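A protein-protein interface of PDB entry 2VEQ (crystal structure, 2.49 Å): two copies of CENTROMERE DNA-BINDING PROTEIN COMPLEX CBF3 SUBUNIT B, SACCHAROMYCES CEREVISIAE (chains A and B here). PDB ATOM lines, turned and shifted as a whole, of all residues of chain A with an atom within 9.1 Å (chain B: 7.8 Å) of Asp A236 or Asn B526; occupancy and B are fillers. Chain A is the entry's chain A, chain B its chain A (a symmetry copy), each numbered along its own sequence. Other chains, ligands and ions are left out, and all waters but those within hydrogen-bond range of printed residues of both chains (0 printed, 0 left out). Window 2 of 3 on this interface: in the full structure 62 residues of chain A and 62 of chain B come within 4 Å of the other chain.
Among the printed residues, merely in contact across the chains: Val A238 with Val B523, Asp A236 with Pro B524, Ala A242 with Ile B516 and Val A238 with Ile B516.
No position is printed for both chains.
Pro A231 touches none of the printed residues of chain B. Asn A234 touches none of the printed residues of chain B. Of the printed residues of chain B, Asp A236 touches Pro B524 (3.7 Å), Leu B525 (3.1 Å) and Asn B526 (3.2 Å). Pro A237 touches none of the printed residues of chain B. Printed residues of chain B within 4 Å of Ala A242: Ile B516. Of the printed residues of chain A, Ile B516 touches Val A238 and Ala A242. Of the printed residues of chain A, Val B523 touches Val A238. Of the printed residues of chain A, Pro B524 touches Asp A236 (3.7 Å). Of chain A, only Asp A236 (3.1 Å) comes within 4 Å of Leu B525. Asn B526 touches one residue of chain A. The nearest residue of chain B that does not touch Asp A236 is Val B523 (5.5 Å). The nearest residue of chain A that does not touch Asn B526 is Pro A237 (4.8 Å).
The side-chain carboxylate (OD2) of Asp A236 is in hydrogen-bond range of the backbone NH (N) of Leu B525 (3.1 Å). ND2 of Asn B526 is in hydrogen-bond range of OD2 of Asp A236, 3.2 Å away.
Of the 6 printed residues of chain B, 5 touch a printed residue of chain A. Hydrophobic or aromatic side chains of chain B within 4 Å of the printed part of chain A: Ile B516 and Pro B524. Hydrophobic or aromatic side chains of chain A within 4 Å of the printed part of chain B: Val A238 and Ala A242.
The backbone NH of Val A238 lies within hydrogen-bond range of the side-chain carboxylate of Asp A236.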
ATOM      1  N   PRO A 231     -21.071  16.705  12.906  1.00  0.00           N
ATOM      2  CA  PRO A 231     -20.003  16.379  11.954  1.00  0.00           C
ATOM      3  C   PRO A 231     -19.199  15.174  12.440  1.00  0.00           C
ATOM      4  O   PRO A 231     -18.928  15.048  13.632  1.00  0.00           O
ATOM      5  CB  PRO A 231     -19.159  17.651  11.934  1.00  0.00           C
ATOM      6  CG  PRO A 231     -20.147  18.718  12.283  1.00  0.00           C
ATOM      7  CD  PRO A 231     -20.925  18.083  13.398  1.00  0.00           C
ATOM      8  N   LEU A 232     -18.819  14.297  11.518  1.00  0.00           N
ATOM      9  CA  LEU A 232     -18.052  13.110  11.880  1.00  0.00           C
ATOM     10  C   LEU A 232     -16.618  13.167  11.349  1.00  0.00           C
ATOM     11  O   LEU A 232     -16.356  13.749  10.292  1.00  0.00           O
ATOM     12  CB  LEU A 232     -18.769  11.861  11.365  1.00  0.00           C
ATOM     13  CG  LEU A 232     -20.227  11.781  11.838  1.00  0.00           C
ATOM     14  CD1 LEU A 232     -20.903  10.551  11.243  1.00  0.00           C
ATOM     15  CD2 LEU A 232     -20.274  11.751  13.366  1.00  0.00           C
ATOM     16  N   LEU A 233     -15.695  12.567  12.101  1.00  0.00           N
ATOM     17  CA  LEU A 233     -14.278  12.549  11.739  1.00  0.00           C
ATOM     18  C   LEU A 233     -14.051  12.047  10.319  1.00  0.00           C
ATOM     19  O   LEU A 233     -13.218  12.583   9.583  1.00  0.00           O
ATOM     20  CB  LEU A 233     -13.494  11.683  12.732  1.00  0.00           C
ATOM     21  N   ASN A 234     -14.799  11.020   9.932  1.00  0.00           N
ATOM     22  CA  ASN A 234     -14.660  10.451   8.598  1.00  0.00           C
ATOM     23  C   ASN A 234     -15.410  11.246   7.526  1.00  0.00           C
ATOM     24  O   ASN A 234     -15.466  10.829   6.371  1.00  0.00           O
ATOM     25  CB  ASN A 234     -15.144   8.995   8.611  1.00  0.00           C
ATOM     26  N   ASP A 235     -15.974  12.393   7.898  1.00  0.00           N
ATOM     27  CA  ASP A 235     -16.731  13.204   6.947  1.00  0.00           C
ATOM     28  C   ASP A 235     -15.952  14.222   6.135  1.00  0.00           C
ATOM     29  O   ASP A 235     -14.997  14.837   6.607  1.00  0.00           O
ATOM     30  CB  ASP A 235     -17.865  13.961   7.654  1.00  0.00           C
ATOM     31  CG  ASP A 235     -19.159  13.177   7.706  1.00  0.00           C
ATOM     32  OD1 ASP A 235     -19.207  12.059   7.149  1.00  0.00           O
ATOM     33  OD2 ASP A 235     -20.134  13.688   8.292  1.00  0.00           O
ATOM     34  N   ASP A 236     -16.387  14.399   4.897  1.00  0.00           N
ATOM     35  CA  ASP A 236     -15.798  15.389   4.018  1.00  0.00           C
ATOM     36  C   ASP A 236     -16.316  16.694   4.622  1.00  0.00           C
ATOM     37  O   ASP A 236     -17.491  16.783   4.990  1.00  0.00           O
ATOM     38  CB  ASP A 236     -16.354  15.231   2.603  1.00  0.00           C
ATOM     39  CG  ASP A 236     -15.741  16.205   1.625  1.00  0.00           C
ATOM     40  OD1 ASP A 236     -15.474  17.364   2.025  1.00  0.00           O
ATOM     41  OD2 ASP A 236     -15.534  15.820   0.453  1.00  0.00           O
ATOM     42  N   PRO A 237     -15.450  17.714   4.757  1.00  0.00           N
ATOM     43  CA  PRO A 237     -15.895  18.989   5.329  1.00  0.00           C
ATOM     44  C   PRO A 237     -17.161  19.539   4.667  1.00  0.00           C
ATOM     45  O   PRO A 237     -18.031  20.079   5.341  1.00  0.00           O
ATOM     46  CB  PRO A 237     -14.677  19.886   5.127  1.00  0.00           C
ATOM     47  CG  PRO A 237     -13.547  18.917   5.352  1.00  0.00           C
ATOM     48  CD  PRO A 237     -13.991  17.722   4.538  1.00  0.00           C
ATOM     49  N   VAL A 238     -17.258  19.398   3.349  1.00  0.00           N
ATOM     50  CA  VAL A 238     -18.428  19.871   2.615  1.00  0.00           C
ATOM     51  C   VAL A 238     -19.685  19.145   3.084  1.00  0.00           C
ATOM     52  O   VAL A 238     -20.779  19.714   3.106  1.00  0.00           O
ATOM     53  CB  VAL A 238     -18.266  19.637   1.101  1.00  0.00           C
ATOM     54  CG1 VAL A 238     -19.558  20.005   0.368  1.00  0.00           C
ATOM     55  CG2 VAL A 238     -17.117  20.472   0.577  1.00  0.00           C
ATOM     56  N   GLU A 239     -19.514  17.884   3.461  1.00  0.00           N
ATOM     57  CA  GLU A 239     -20.606  17.051   3.933  1.00  0.00           C
ATOM     58  C   GLU A 239     -20.956  17.421   5.373  1.00  0.00           C
ATOM     59  O   GLU A 239     -22.120  17.371   5.769  1.00  0.00           O
ATOM     60  CB  GLU A 239     -20.187  15.587   3.849  1.00  0.00           C
ATOM     61  CG  GLU A 239     -21.315  14.590   3.886  1.00  0.00           C
ATOM     62  CD  GLU A 239     -20.806  13.161   3.763  1.00  0.00           C
ATOM     63  OE1 GLU A 239     -19.763  12.958   3.086  1.00  0.00           O
ATOM     64  OE2 GLU A 239     -21.450  12.249   4.332  1.00  0.00           O
ATOM     65  N   SER A 240     -19.948  17.794   6.156  1.00  0.00           N
ATOM     66  CA  SER A 240     -20.176  18.188   7.540  1.00  0.00           C
ATOM     67  C   SER A 240     -20.952  19.502   7.590  1.00  0.00           C
ATOM     68  O   SER A 240     -21.795  19.708   8.460  1.00  0.00           O
ATOM     69  CB  SER A 240     -18.846  18.359   8.275  1.00  0.00           C
ATOM     70  OG  SER A 240     -18.192  17.112   8.453  1.00  0.00           O
ATOM     71  N   ILE A 241     -20.653  20.383   6.642  1.00  0.00           N
ATOM     72  CA  ILE A 241     -21.296  21.687   6.547  1.00  0.00           C
ATOM     73  C   ILE A 241     -22.754  21.534   6.112  1.00  0.00           C
ATOM     74  O   ILE A 241     -23.643  22.249   6.590  1.00  0.00           O
ATOM     75  CB  ILE A 241     -20.547  22.592   5.529  1.00  0.00           C
ATOM     76  CG1 ILE A 241     -19.142  22.913   6.060  1.00  0.00           C
ATOM     77  CG2 ILE A 241     -21.370  23.842   5.238  1.00  0.00           C
ATOM     78  CD1 ILE A 241     -18.269  23.757   5.102  1.00  0.00           C
ATOM     79  N   ALA A 242     -22.994  20.610   5.191  1.00  0.00           N
ATOM     80  CA  ALA A 242     -24.343  20.366   4.717  1.00  0.00           C
ATOM     81  C   ALA A 242     -25.224  19.835   5.855  1.00  0.00           C
ATOM     82  O   ALA A 242     -26.404  20.159   5.920  1.00  0.00           O
ATOM     83  CB  ALA A 242     -24.323  19.370   3.554  1.00  0.00           C
ATOM     84  N   LYS A 243     -24.646  19.041   6.755  1.00  0.00           N
ATOM     85  CA  LYS A 243     -25.405  18.469   7.861  1.00  0.00           C
ATOM     86  C   LYS A 243     -25.677  19.455   8.990  1.00  0.00           C
ATOM     87  O   LYS A 243     -26.731  19.393   9.637  1.00  0.00           O
ATOM     88  CB  LYS A 243     -24.701  17.219   8.407  1.00  0.00           C
ATOM     89  CG  LYS A 243     -24.558  16.110   7.352  1.00  0.00           C
ATOM     90  CD  LYS A 243     -24.199  14.758   7.951  1.00  0.00           C
ATOM     91  CE  LYS A 243     -22.847  14.772   8.626  1.00  0.00           C
ATOM     92  NZ  LYS A 243     -22.478  13.421   9.117  1.00  0.00           N
ATOM     93  N   PHE B 513     -25.879  13.985  -1.945  1.00  0.00           N
ATOM     94  CA  PHE B 513     -25.373  14.703  -3.106  1.00  0.00           C
ATOM     95  C   PHE B 513     -26.305  15.829  -3.510  1.00  0.00           C
ATOM     96  O   PHE B 513     -25.867  16.963  -3.703  1.00  0.00           O
ATOM     97  CB  PHE B 513     -25.191  13.749  -4.289  1.00  0.00           C
ATOM     98  CG  PHE B 513     -24.225  12.639  -4.020  1.00  0.00           C
ATOM     99  CD1 PHE B 513     -22.866  12.911  -3.849  1.00  0.00           C
ATOM    100  CD2 PHE B 513     -24.673  11.322  -3.914  1.00  0.00           C
ATOM    101  CE1 PHE B 513     -21.955  11.881  -3.573  1.00  0.00           C
ATOM    102  CE2 PHE B 513     -23.777  10.280  -3.638  1.00  0.00           C
ATOM    103  CZ  PHE B 513     -22.413  10.559  -3.465  1.00  0.00           C
ATOM    104  N   ILE B 516     -26.182  18.695  -0.871  1.00  0.00           N
ATOM    105  CA  ILE B 516     -25.013  19.535  -1.072  1.00  0.00           C
ATOM    106  C   ILE B 516     -25.192  20.470  -2.269  1.00  0.00           C
ATOM    107  O   ILE B 516     -24.819  21.637  -2.203  1.00  0.00           O
ATOM    108  CB  ILE B 516     -23.761  18.648  -1.265  1.00  0.00           C
ATOM    109  CG1 ILE B 516     -23.341  18.070   0.091  1.00  0.00           C
ATOM    110  CG2 ILE B 516     -22.633  19.436  -1.932  1.00  0.00           C
ATOM    111  CD1 ILE B 516     -22.375  16.900  -0.001  1.00  0.00           C
ATOM    112  N   VAL B 523     -18.589  21.917  -3.515  1.00  0.00           N
ATOM    113  CA  VAL B 523     -18.543  20.607  -4.152  1.00  0.00           C
ATOM    114  C   VAL B 523     -17.643  19.669  -3.345  1.00  0.00           C
ATOM    115  O   VAL B 523     -16.534  20.039  -2.952  1.00  0.00           O
ATOM    116  CB  VAL B 523     -17.999  20.708  -5.601  1.00  0.00           C
ATOM    117  CG1 VAL B 523     -17.975  19.329  -6.248  1.00  0.00           C
ATOM    118  CG2 VAL B 523     -18.867  21.657  -6.419  1.00  0.00           C
ATOM    119  N   PRO B 524     -18.108  18.450  -3.073  1.00  0.00           N
ATOM    120  CA  PRO B 524     -17.220  17.543  -2.324  1.00  0.00           C
ATOM    121  C   PRO B 524     -16.001  17.086  -3.096  1.00  0.00           C
ATOM    122  O   PRO B 524     -16.055  16.910  -4.323  1.00  0.00           O
ATOM    123  CB  PRO B 524     -18.153  16.321  -2.121  1.00  0.00           C
ATOM    124  CG  PRO B 524     -19.045  16.352  -3.331  1.00  0.00           C
ATOM    125  CD  PRO B 524     -19.311  17.834  -3.519  1.00  0.00           C
ATOM    126  N   LEU B 525     -14.895  16.891  -2.385  1.00  0.00           N
ATOM    127  CA  LEU B 525     -13.694  16.316  -2.979  1.00  0.00           C
ATOM    128  C   LEU B 525     -13.666  14.800  -2.808  1.00  0.00           C
ATOM    129  O   LEU B 525     -14.107  14.058  -3.686  1.00  0.00           O
ATOM    130  CB  LEU B 525     -12.440  16.937  -2.361  1.00  0.00           C
ATOM    131  N   ASN B 526     -13.146  14.348  -1.672  1.00  0.00           N
ATOM    132  CA  ASN B 526     -13.362  12.978  -1.221  1.00  0.00           C
ATOM    133  C   ASN B 526     -14.672  12.399  -1.747  1.00  0.00           C
ATOM    134  O   ASN B 526     -14.812  11.185  -1.887  1.00  0.00           O
ATOM    135  CB  ASN B 526     -13.329  12.904   0.306  1.00  0.00           C
ATOM    136  CG  ASN B 526     -12.270  13.804   0.911  1.00  0.00           C
ATOM    137  OD1 ASN B 526     -11.288  13.329   1.482  1.00  0.00           O
ATOM    138  ND2 ASN B 526     -12.465  15.111   0.789  1.00  0.00           N
